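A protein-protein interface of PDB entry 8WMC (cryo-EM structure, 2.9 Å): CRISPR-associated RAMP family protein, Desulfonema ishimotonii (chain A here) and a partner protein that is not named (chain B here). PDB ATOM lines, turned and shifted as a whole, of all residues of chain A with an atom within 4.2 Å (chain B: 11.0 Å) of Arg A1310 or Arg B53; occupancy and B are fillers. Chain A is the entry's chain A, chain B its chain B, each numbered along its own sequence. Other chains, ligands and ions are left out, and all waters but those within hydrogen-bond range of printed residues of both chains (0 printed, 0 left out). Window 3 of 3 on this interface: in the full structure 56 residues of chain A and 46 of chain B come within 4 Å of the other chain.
The backbone NH of Gly B49 is in hydrogen-bond range of the backbone carbonyl oxygen of His A1337, 2.7 Å away. The guanidinium group of Arg B53 sits close to the guanidinium group of Arg A1310 (3.4 Å). NH2 of Arg B53 is in hydrogen-bond range of O of Arg A1336, at 3.2 Å.
The guanidinium group (NE) of Arg A1310 lies within salt-bridge range of the side-chain carboxylate (OE2) of Glu A971 (3.9 Å). A ring nitrogen (ND1) of His A1337 sits at hydrogen-bond distance from the guanidinium group (NE) of Arg A876 (3.2 Å). The backbone NH (N) of His A1337 lies within hydrogen-bond range of the backbone carbonyl oxygen (O) of Cys A1312, 3.3 Å away.
Among the printed residues, pairs that only touch across the chains: Leu A1334 with Arg B53 (3.7 Å), Leu A1335 with Arg B53 (3.8 Å), Arg A1336 with Gln B47 (3.8 Å), Arg A1336 with Gln B48 (3.9 Å), Arg A1336 with Gly B49 (3.8 Å), His A1337 with Gln B48 (3.2 Å) and His A1337 with Arg B53 (3.9 Å).
No residue of chain B comes within 4 Å of Cys A965. No residue of chain B comes within 4 Å of Gly A1302. No residue of chain B comes within 4 Å of Met A1305. No residue of chain B comes within 4 Å of Leu A1309. Arg A1310 touches one residue of chain B. No residue of chain B comes within 4 Å of Pro A1311. No residue of chain B comes within 4 Å of Cys A1312. His A1337 touches just these residues of chain B: Gln B48, Gly B49 and Arg B53. Of the printed residues of chain A, Gln B47 touches Arg A1336. Of the printed residues of chain A, Gln B48 touches Arg A1336 (3.9 Å) and His A1337 (3.2 Å). The nearest printed residue of chain A that does not touch Arg B53 is Cys A1312 (5.0 Å). The nearest printed residue of chain A that does not touch Gln B47 is His A1337 (4.3 Å).
Among the printed residues, no Asp or Glu carboxylate lies within 4 Å of a Lys or Arg side-chain nitrogen of the other chain.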
ATOM      1  N   ARG A 876      -3.900   5.199  -7.376  1.00  0.00           N
ATOM      2  CA  ARG A 876      -4.581   6.029  -8.357  1.00  0.00           C
ATOM      3  C   ARG A 876      -5.323   5.169  -9.375  1.00  0.00           C
ATOM      4  O   ARG A 876      -5.085   3.967  -9.503  1.00  0.00           O
ATOM      5  CB  ARG A 876      -3.582   6.937  -9.075  1.00  0.00           C
ATOM      6  CG  ARG A 876      -2.723   7.761  -8.137  1.00  0.00           C
ATOM      7  CD  ARG A 876      -2.473   9.148  -8.694  1.00  0.00           C
ATOM      8  NE  ARG A 876      -1.358   9.809  -8.018  1.00  0.00           N
ATOM      9  CZ  ARG A 876      -1.446  10.830  -7.170  1.00  0.00           C
ATOM     10  NH1 ARG A 876      -2.610  11.349  -6.808  1.00  0.00           N
ATOM     11  NH2 ARG A 876      -0.329  11.344  -6.664  1.00  0.00           N
ATOM     12  N   CYS A 965      -3.584  12.165  -1.662  1.00  0.00           N
ATOM     13  CA  CYS A 965      -2.687  13.275  -1.927  1.00  0.00           C
ATOM     14  C   CYS A 965      -3.050  14.476  -1.058  1.00  0.00           C
ATOM     15  O   CYS A 965      -4.128  14.549  -0.463  1.00  0.00           O
ATOM     16  CB  CYS A 965      -2.740  13.663  -3.403  1.00  0.00           C
ATOM     17  SG  CYS A 965      -4.209  14.617  -3.882  1.00  0.00           S
ATOM     18  N   GLU A 971       1.984  25.257  -3.920  1.00  0.00           N
ATOM     19  CA  GLU A 971       3.183  24.756  -4.585  1.00  0.00           C
ATOM     20  C   GLU A 971       4.159  25.865  -4.956  1.00  0.00           C
ATOM     21  O   GLU A 971       5.372  25.632  -4.975  1.00  0.00           O
ATOM     22  CB  GLU A 971       2.793  23.987  -5.846  1.00  0.00           C
ATOM     23  CG  GLU A 971       2.039  22.698  -5.593  1.00  0.00           C
ATOM     24  CD  GLU A 971       1.662  21.995  -6.879  1.00  0.00           C
ATOM     25  OE1 GLU A 971       1.883  22.576  -7.961  1.00  0.00           O
ATOM     26  OE2 GLU A 971       1.149  20.861  -6.814  1.00  0.00           O
ATOM     27  N   GLY A1302       7.101  22.947  -3.717  1.00  0.00           N
ATOM     28  CA  GLY A1302       6.524  21.757  -4.315  1.00  0.00           C
ATOM     29  C   GLY A1302       7.532  20.671  -4.630  1.00  0.00           C
ATOM     30  O   GLY A1302       7.153  19.501  -4.729  1.00  0.00           O
ATOM     31  N   MET A1305       8.815  17.657  -1.534  1.00  0.00           N
ATOM     32  CA  MET A1305       8.028  16.510  -1.108  1.00  0.00           C
ATOM     33  C   MET A1305       7.960  15.500  -2.245  1.00  0.00           C
ATOM     34  O   MET A1305       8.291  15.804  -3.394  1.00  0.00           O
ATOM     35  CB  MET A1305       6.618  16.937  -0.665  1.00  0.00           C
ATOM     36  CG  MET A1305       5.739  17.528  -1.763  1.00  0.00           C
ATOM     37  SD  MET A1305       4.108  17.984  -1.148  1.00  0.00           S
ATOM     38  CE  MET A1305       3.368  16.373  -0.906  1.00  0.00           C
ATOM     39  N   SER A1306       7.540  14.284  -1.904  1.00  0.00           N
ATOM     40  CA  SER A1306       7.441  13.223  -2.898  1.00  0.00           C
ATOM     41  C   SER A1306       6.442  13.598  -3.983  1.00  0.00           C
ATOM     42  O   SER A1306       5.375  14.153  -3.706  1.00  0.00           O
ATOM     43  CB  SER A1306       7.026  11.912  -2.231  1.00  0.00           C
ATOM     44  OG  SER A1306       6.953  10.860  -3.178  1.00  0.00           O
ATOM     45  N   ALA A1307       6.797  13.292  -5.233  1.00  0.00           N
ATOM     46  CA  ALA A1307       5.938  13.636  -6.359  1.00  0.00           C
ATOM     47  C   ALA A1307       4.600  12.911  -6.311  1.00  0.00           C
ATOM     48  O   ALA A1307       3.619  13.408  -6.874  1.00  0.00           O
ATOM     49  CB  ALA A1307       6.649  13.321  -7.674  1.00  0.00           C
ATOM     50  N   ASP A1308       4.535  11.749  -5.659  1.00  0.00           N
ATOM     51  CA  ASP A1308       3.276  11.017  -5.584  1.00  0.00           C
ATOM     52  C   ASP A1308       2.267  11.717  -4.685  1.00  0.00           C
ATOM     53  O   ASP A1308       1.058  11.622  -4.925  1.00  0.00           O
ATOM     54  CB  ASP A1308       3.528   9.596  -5.084  1.00  0.00           C
ATOM     55  CG  ASP A1308       4.319   8.760  -6.070  1.00  0.00           C
ATOM     56  OD1 ASP A1308       4.119   8.926  -7.292  1.00  0.00           O
ATOM     57  OD2 ASP A1308       5.144   7.934  -5.623  1.00  0.00           O
ATOM     58  N   LEU A1309       2.733  12.421  -3.655  1.00  0.00           N
ATOM     59  CA  LEU A1309       1.855  13.039  -2.671  1.00  0.00           C
ATOM     60  C   LEU A1309       1.396  14.438  -3.061  1.00  0.00           C
ATOM     61  O   LEU A1309       0.604  15.037  -2.326  1.00  0.00           O
ATOM     62  CB  LEU A1309       2.557  13.096  -1.312  1.00  0.00           C
ATOM     63  CG  LEU A1309       2.779  11.747  -0.627  1.00  0.00           C
ATOM     64  CD1 LEU A1309       3.833  11.871   0.459  1.00  0.00           C
ATOM     65  CD2 LEU A1309       1.478  11.203  -0.053  1.00  0.00           C
ATOM     66  N   ARG A1310       1.862  14.977  -4.185  1.00  0.00           N
ATOM     67  CA  ARG A1310       1.403  16.280  -4.624  1.00  0.00           C
ATOM     68  C   ARG A1310      -0.032  16.179  -5.140  1.00  0.00           C
ATOM     69  O   ARG A1310      -0.517  15.080  -5.419  1.00  0.00           O
ATOM     70  CB  ARG A1310       2.314  16.831  -5.716  1.00  0.00           C
ATOM     71  CG  ARG A1310       3.545  17.546  -5.191  1.00  0.00           C
ATOM     72  CD  ARG A1310       4.609  17.671  -6.265  1.00  0.00           C
ATOM     73  NE  ARG A1310       4.129  18.408  -7.428  1.00  0.00           N
ATOM     74  CZ  ARG A1310       4.773  18.506  -8.585  1.00  0.00           C
ATOM     75  NH1 ARG A1310       5.942  17.918  -8.784  1.00  0.00           N
ATOM     76  NH2 ARG A1310       4.229  19.216  -9.569  1.00  0.00           N
ATOM     77  N   PRO A1311      -0.739  17.307  -5.259  1.00  0.00           N
ATOM     78  CA  PRO A1311      -2.103  17.259  -5.801  1.00  0.00           C
ATOM     79  C   PRO A1311      -2.128  16.674  -7.206  1.00  0.00           C
ATOM     80  O   PRO A1311      -1.211  16.884  -8.003  1.00  0.00           O
ATOM     81  CB  PRO A1311      -2.547  18.726  -5.802  1.00  0.00           C
ATOM     82  CG  PRO A1311      -1.635  19.434  -4.890  1.00  0.00           C
ATOM     83  CD  PRO A1311      -0.368  18.656  -4.798  1.00  0.00           C
ATOM     84  N   CYS A1312      -3.204  15.959  -7.536  1.00  0.00           N
ATOM     85  CA  CYS A1312      -3.360  15.286  -8.841  1.00  0.00           C
ATOM     86  C   CYS A1312      -3.369  16.377  -9.906  1.00  0.00           C
ATOM     87  O   CYS A1312      -2.425  16.389 -10.703  1.00  0.00           O
ATOM     88  CB  CYS A1312      -4.648  14.465  -8.890  1.00  0.00           C
ATOM     89  SG  CYS A1312      -4.871  13.258  -7.556  1.00  0.00           S
ATOM     90  N   ASP A1315      -0.341  22.691  -9.982  1.00  0.00           N
ATOM     91  CA  ASP A1315       0.253  23.784 -10.734  1.00  0.00           C
ATOM     92  C   ASP A1315       1.552  23.313 -11.383  1.00  0.00           C
ATOM     93  O   ASP A1315       1.993  22.175 -11.197  1.00  0.00           O
ATOM     94  CB  ASP A1315       0.500  24.990  -9.821  1.00  0.00           C
ATOM     95  CG  ASP A1315      -0.786  25.647  -9.359  1.00  0.00           C
ATOM     96  OD1 ASP A1315      -1.792  25.587 -10.097  1.00  0.00           O
ATOM     97  OD2 ASP A1315      -0.790  26.230  -8.254  1.00  0.00           O
ATOM     98  N   VAL A1317       5.467  23.576 -11.606  1.00  0.00           N
ATOM     99  CA  VAL A1317       6.608  23.929 -10.767  1.00  0.00           C
ATOM    100  C   VAL A1317       7.946  23.679 -11.445  1.00  0.00           C
ATOM    101  O   VAL A1317       8.977  24.134 -10.925  1.00  0.00           O
ATOM    102  CB  VAL A1317       6.563  23.188  -9.410  1.00  0.00           C
ATOM    103  CG1 VAL A1317       5.320  23.581  -8.633  1.00  0.00           C
ATOM    104  CG2 VAL A1317       6.624  21.669  -9.595  1.00  0.00           C
ATOM    105  N   LEU A1334      -0.119  18.708 -19.269  1.00  0.00           N
ATOM    106  CA  LEU A1334       1.150  18.892 -18.578  1.00  0.00           C
ATOM    107  C   LEU A1334       0.987  19.198 -17.093  1.00  0.00           C
ATOM    108  O   LEU A1334       1.999  19.329 -16.397  1.00  0.00           O
ATOM    109  CB  LEU A1334       1.946  20.019 -19.243  1.00  0.00           C
ATOM    110  CG  LEU A1334       2.518  19.724 -20.632  1.00  0.00           C
ATOM    111  CD1 LEU A1334       3.036  20.999 -21.271  1.00  0.00           C
ATOM    112  CD2 LEU A1334       3.621  18.680 -20.561  1.00  0.00           C
ATOM    113  N   LEU A1335      -0.247  19.319 -16.596  1.00  0.00           N
ATOM    114  CA  LEU A1335      -0.518  19.595 -15.191  1.00  0.00           C
ATOM    115  C   LEU A1335      -1.092  18.407 -14.436  1.00  0.00           C
ATOM    116  O   LEU A1335      -0.904  18.317 -13.222  1.00  0.00           O
ATOM    117  CB  LEU A1335      -1.493  20.773 -15.061  1.00  0.00           C
ATOM    118  CG  LEU A1335      -1.032  22.103 -15.664  1.00  0.00           C
ATOM    119  CD1 LEU A1335      -2.198  23.068 -15.774  1.00  0.00           C
ATOM    120  CD2 LEU A1335       0.091  22.715 -14.847  1.00  0.00           C
ATOM    121  N   ARG A1336      -1.781  17.497 -15.118  1.00  0.00           N
ATOM    122  CA  ARG A1336      -2.395  16.357 -14.458  1.00  0.00           C
ATOM    123  C   ARG A1336      -1.359  15.269 -14.188  1.00  0.00           C
ATOM    124  O   ARG A1336      -0.287  15.226 -14.798  1.00  0.00           O
ATOM    125  CB  ARG A1336      -3.535  15.791 -15.308  1.00  0.00           C
ATOM    126  CG  ARG A1336      -4.440  16.850 -15.918  1.00  0.00           C
ATOM    127  CD  ARG A1336      -5.708  16.252 -16.500  1.00  0.00           C
ATOM    128  NE  ARG A1336      -6.749  17.258 -16.677  1.00  0.00           N
ATOM    129  CZ  ARG A1336      -7.969  17.015 -17.142  1.00  0.00           C
ATOM    130  NH1 ARG A1336      -8.350  15.799 -17.500  1.00  0.00           N
ATOM    131  NH2 ARG A1336      -8.830  18.022 -17.251  1.00  0.00           N
ATOM    132  N   HIS A1337      -1.693  14.383 -13.253  1.00  0.00           N
ATOM    133  CA  HIS A1337      -0.794  13.296 -12.910  1.00  0.00           C
ATOM    134  C   HIS A1337      -0.816  12.233 -14.014  1.00  0.00           C
ATOM    135  O   HIS A1337      -1.844  12.036 -14.665  1.00  0.00           O
ATOM    136  CB  HIS A1337      -1.198  12.670 -11.578  1.00  0.00           C
ATOM    137  CG  HIS A1337      -0.102  11.896 -10.918  1.00  0.00           C
ATOM    138  ND1 HIS A1337      -0.077  10.518 -10.890  1.00  0.00           N
ATOM    139  CD2 HIS A1337       1.013  12.304 -10.269  1.00  0.00           C
ATOM    140  CE1 HIS A1337       1.004  10.112 -10.250  1.00  0.00           C
ATOM    141  NE2 HIS A1337       1.683  11.176  -9.862  1.00  0.00           N
ATOM    142  N   GLN B   9       1.508  10.045 -26.003  1.00  0.00           N
ATOM    143  CA  GLN B   9       2.751   9.719 -25.311  1.00  0.00           C
ATOM    144  C   GLN B   9       3.648   8.843 -26.178  1.00  0.00           C
ATOM    145  O   GLN B   9       4.865   9.063 -26.249  1.00  0.00           O
ATOM    146  CB  GLN B   9       2.436   9.025 -23.984  1.00  0.00           C
ATOM    147  CG  GLN B   9       3.638   8.806 -23.067  1.00  0.00           C
ATOM    148  CD  GLN B   9       4.219  10.102 -22.538  1.00  0.00           C
ATOM    149  OE1 GLN B   9       3.486  10.997 -22.118  1.00  0.00           O
ATOM    150  NE2 GLN B   9       5.542  10.211 -22.558  1.00  0.00           N
ATOM    151  N   LEU B  12       5.167  10.981 -28.894  1.00  0.00           N
ATOM    152  CA  LEU B  12       6.167  11.888 -28.341  1.00  0.00           C
ATOM    153  C   LEU B  12       7.443  11.153 -27.952  1.00  0.00           C
ATOM    154  O   LEU B  12       8.525  11.753 -27.959  1.00  0.00           O
ATOM    155  CB  LEU B  12       5.597  12.623 -27.128  1.00  0.00           C
ATOM    156  CG  LEU B  12       4.836  13.914 -27.429  1.00  0.00           C
ATOM    157  CD1 LEU B  12       3.922  14.273 -26.273  1.00  0.00           C
ATOM    158  CD2 LEU B  12       5.798  15.052 -27.730  1.00  0.00           C
ATOM    159  N   GLN B  47      -8.490  10.971 -16.992  1.00  0.00           N
ATOM    160  CA  GLN B  47      -8.032  12.080 -16.160  1.00  0.00           C
ATOM    161  C   GLN B  47      -6.546  11.958 -15.848  1.00  0.00           C
ATOM    162  O   GLN B  47      -6.109  12.253 -14.732  1.00  0.00           O
ATOM    163  CB  GLN B  47      -8.830  12.155 -14.856  1.00  0.00           C
ATOM    164  CG  GLN B  47     -10.349  12.308 -15.013  1.00  0.00           C
ATOM    165  CD  GLN B  47     -10.817  13.753 -15.041  1.00  0.00           C
ATOM    166  OE1 GLN B  47     -10.208  14.635 -14.438  1.00  0.00           O
ATOM    167  NE2 GLN B  47     -11.914  13.997 -15.746  1.00  0.00           N
ATOM    168  N   GLN B  48      -5.747  11.528 -16.822  1.00  0.00           N
ATOM    169  CA  GLN B  48      -4.300  11.408 -16.674  1.00  0.00           C
ATOM    170  C   GLN B  48      -3.589  12.471 -17.504  1.00  0.00           C
ATOM    171  O   GLN B  48      -4.199  13.194 -18.295  1.00  0.00           O
ATOM    172  CB  GLN B  48      -3.826   9.985 -17.038  1.00  0.00           C
ATOM    173  CG  GLN B  48      -3.644   9.612 -18.527  1.00  0.00           C
ATOM    174  CD  GLN B  48      -4.789   8.778 -19.055  1.00  0.00           C
ATOM    175  OE1 GLN B  48      -5.951   9.042 -18.756  1.00  0.00           O
ATOM    176  NE2 GLN B  48      -4.468   7.769 -19.856  1.00  0.00           N
ATOM    177  N   GLY B  49      -2.273  12.549 -17.303  1.00  0.00           N
ATOM    178  CA  GLY B  49      -1.418  13.483 -18.013  1.00  0.00           C
ATOM    179  C   GLY B  49      -0.307  12.781 -18.764  1.00  0.00           C
ATOM    180  O   GLY B  49      -0.411  11.588 -19.059  1.00  0.00           O
ATOM    181  N   LEU B  50       0.762  13.512 -19.073  1.00  0.00           N
ATOM    182  CA  LEU B  50       1.895  12.994 -19.828  1.00  0.00           C
ATOM    183  C   LEU B  50       3.095  12.842 -18.904  1.00  0.00           C
ATOM    184  O   LEU B  50       3.421  13.763 -18.146  1.00  0.00           O
ATOM    185  CB  LEU B  50       2.249  13.924 -20.991  1.00  0.00           C
ATOM    186  CG  LEU B  50       1.189  14.130 -22.076  1.00  0.00           C
ATOM    187  CD1 LEU B  50       1.671  15.161 -23.082  1.00  0.00           C
ATOM    188  CD2 LEU B  50       0.837  12.826 -22.776  1.00  0.00           C
ATOM    189  N   SER B  51       3.745  11.684 -18.970  1.00  0.00           N
ATOM    190  CA  SER B  51       4.943  11.435 -18.185  1.00  0.00           C
ATOM    191  C   SER B  51       6.140  12.151 -18.804  1.00  0.00           C
ATOM    192  O   SER B  51       6.117  12.564 -19.966  1.00  0.00           O
ATOM    193  CB  SER B  51       5.215   9.934 -18.090  1.00  0.00           C
ATOM    194  OG  SER B  51       6.353   9.669 -17.291  1.00  0.00           O
ATOM    195  N   ASN B  52       7.200  12.290 -18.007  1.00  0.00           N
ATOM    196  CA  ASN B  52       8.416  12.985 -18.430  1.00  0.00           C
ATOM    197  C   ASN B  52       8.095  14.431 -18.822  1.00  0.00           C
ATOM    198  O   ASN B  52       8.215  14.838 -19.980  1.00  0.00           O
ATOM    199  CB  ASN B  52       9.101  12.226 -19.573  1.00  0.00           C
ATOM    200  CG  ASN B  52      10.591  12.494 -19.637  1.00  0.00           C
ATOM    201  OD1 ASN B  52      11.036  13.632 -19.489  1.00  0.00           O
ATOM    202  ND2 ASN B  52      11.372  11.444 -19.859  1.00  0.00           N
ATOM    203  N   ARG B  53       7.667  15.195 -17.816  1.00  0.00           N
ATOM    204  CA  ARG B  53       7.114  16.527 -18.060  1.00  0.00           C
ATOM    205  C   ARG B  53       8.085  17.483 -18.743  1.00  0.00           C
ATOM    206  O   ARG B  53       7.666  18.164 -19.695  1.00  0.00           O
ATOM    207  CB  ARG B  53       6.603  17.113 -16.739  1.00  0.00           C
ATOM    208  CG  ARG B  53       5.202  16.656 -16.377  1.00  0.00           C
ATOM    209  CD  ARG B  53       4.733  17.269 -15.072  1.00  0.00           C
ATOM    210  NE  ARG B  53       3.596  16.546 -14.513  1.00  0.00           N
ATOM    211  CZ  ARG B  53       3.147  16.677 -13.271  1.00  0.00           C
ATOM    212  NH1 ARG B  53       3.710  17.513 -12.411  1.00  0.00           N
ATOM    213  NH2 ARG B  53       2.105  15.951 -12.879  1.00  0.00           N
ATOM    214  N   PRO B  54       9.351  17.616 -18.324  1.00  0.00           N
ATOM    215  CA  PRO B  54      10.231  18.577 -19.020  1.00  0.00           C
ATOM    216  C   PRO B  54      10.469  18.231 -20.481  1.00  0.00           C
ATOM    217  O   PRO B  54      10.371  19.107 -21.354  1.00  0.00           O
ATOM    218  CB  PRO B  54      11.527  18.522 -18.197  1.00  0.00           C
ATOM    219  CG  PRO B  54      11.140  17.950 -16.886  1.00  0.00           C
ATOM    220  CD  PRO B  54      10.031  16.996 -17.174  1.00  0.00           C
ATOM    221  N   ASN B  55      10.779  16.966 -20.772  1.00  0.00           N
ATOM    222  CA  ASN B  55      11.005  16.552 -22.153  1.00  0.00           C
ATOM    223  C   ASN B  55       9.745  16.724 -22.991  1.00  0.00           C
ATOM    224  O   ASN B  55       9.808  17.207 -24.130  1.00  0.00           O
ATOM    225  CB  ASN B  55      11.476  15.099 -22.184  1.00  0.00           C
ATOM    226  CG  ASN B  55      11.846  14.634 -23.576  1.00  0.00           C
ATOM    227  OD1 ASN B  55      12.919  14.954 -24.085  1.00  0.00           O
ATOM    228  ND2 ASN B  55      10.960  13.864 -24.196  1.00  0.00           N
ATOM    229  N   SER B  56       8.589  16.338 -22.444  1.00  0.00           N
ATOM    230  CA  SER B  56       7.339  16.480 -23.181  1.00  0.00           C
ATOM    231  C   SER B  56       7.026  17.944 -23.458  1.00  0.00           C
ATOM    232  O   SER B  56       6.596  18.295 -24.563  1.00  0.00           O
ATOM    233  CB  SER B  56       6.197  15.826 -22.406  1.00  0.00           C
ATOM    234  OG  SER B  56       6.427  14.440 -22.241  1.00  0.00           O
ATOM    235  N   PHE B  57       7.235  18.814 -22.467  1.00  0.00           N
ATOM    236  CA  PHE B  57       6.983  20.236 -22.668  1.00  0.00           C
ATOM    237  C   PHE B  57       7.910  20.814 -23.726  1.00  0.00           C
ATOM    238  O   PHE B  57       7.475  21.594 -24.581  1.00  0.00           O
ATOM    239  CB  PHE B  57       7.145  20.989 -21.349  1.00  0.00           C
ATOM    240  CG  PHE B  57       7.369  22.463 -21.519  1.00  0.00           C
ATOM    241  CD1 PHE B  57       6.348  23.285 -21.961  1.00  0.00           C
ATOM    242  CD2 PHE B  57       8.601  23.026 -21.239  1.00  0.00           C
ATOM    243  CE1 PHE B  57       6.550  24.640 -22.119  1.00  0.00           C
ATOM    244  CE2 PHE B  57       8.810  24.381 -21.395  1.00  0.00           C
ATOM    245  CZ  PHE B  57       7.782  25.189 -21.835  1.00  0.00           C
ATOM    246  N   SER B  58       9.192  20.443 -23.687  1.00  0.00           N
ATOM    247  CA  SER B  58      10.135  20.946 -24.681  1.00  0.00           C
ATOM    248  C   SER B  58       9.743  20.493 -26.083  1.00  0.00           C
ATOM    249  O   SER B  58       9.749  21.289 -27.032  1.00  0.00           O
ATOM    250  CB  SER B  58      11.549  20.480 -24.341  1.00  0.00           C
ATOM    251  OG  SER B  58      12.465  20.854 -25.355  1.00  0.00           O
ATOM    252  N   GLN B  59       9.388  19.213 -26.229  1.00  0.00           N
ATOM    253  CA  GLN B  59       9.013  18.702 -27.543  1.00  0.00           C
ATOM    254  C   GLN B  59       7.742  19.367 -28.056  1.00  0.00           C
ATOM    255  O   GLN B  59       7.661  19.737 -29.233  1.00  0.00           O
ATOM    256  CB  GLN B  59       8.841  17.185 -27.484  1.00  0.00           C
ATOM    257  CG  GLN B  59      10.151  16.423 -27.587  1.00  0.00           C
ATOM    258  CD  GLN B  59      10.012  14.957 -27.229  1.00  0.00           C
ATOM    259  OE1 GLN B  59      10.824  14.414 -26.481  1.00  0.00           O
ATOM    260  NE2 GLN B  59       8.988  14.304 -27.770  1.00  0.00           N
ATOM    261  N   LEU B  60       6.739  19.533 -27.188  1.00  0.00           N
ATOM    262  CA  LEU B  60       5.502  20.182 -27.609  1.00  0.00           C
ATOM    263  C   LEU B  60       5.748  21.632 -28.005  1.00  0.00           C
ATOM    264  O   LEU B  60       5.206  22.109 -29.010  1.00  0.00           O
ATOM    265  CB  LEU B  60       4.464  20.106 -26.489  1.00  0.00           C
ATOM    266  CG  LEU B  60       3.767  18.759 -26.297  1.00  0.00           C
ATOM    267  CD1 LEU B  60       3.080  18.712 -24.942  1.00  0.00           C
ATOM    268  CD2 LEU B  60       2.769  18.490 -27.412  1.00  0.00           C
ATOM    269  N   SER B  61       6.562  22.351 -27.226  1.00  0.00           N
ATOM    270  CA  SER B  61       6.858  23.740 -27.551  1.00  0.00           C
ATOM    271  C   SER B  61       7.579  23.849 -28.886  1.00  0.00           C
ATOM    272  O   SER B  61       7.241  24.706 -29.713  1.00  0.00           O
ATOM    273  CB  SER B  61       7.696  24.368 -26.438  1.00  0.00           C
ATOM    274  OG  SER B  61       7.729  25.779 -26.558  1.00  0.00           O
ATOM    275  N   GLN B  62       8.569  22.984 -29.124  1.00  0.00           N
ATOM    276  CA  GLN B  62       9.291  23.031 -30.391  1.00  0.00           C
ATOM    277  C   GLN B  62       8.376  22.686 -31.559  1.00  0.00           C
ATOM    278  O   GLN B  62       8.437  23.327 -32.615  1.00  0.00           O
ATOM    279  CB  GLN B  62      10.491  22.087 -30.351  1.00  0.00           C
ATOM    280  CG  GLN B  62      11.759  22.728 -29.814  1.00  0.00           C
ATOM    281  CD  GLN B  62      12.842  21.715 -29.503  1.00  0.00           C
ATOM    282  OE1 GLN B  62      12.717  20.537 -29.834  1.00  0.00           O
ATOM    283  NE2 GLN B  62      13.912  22.170 -28.862  1.00  0.00           N
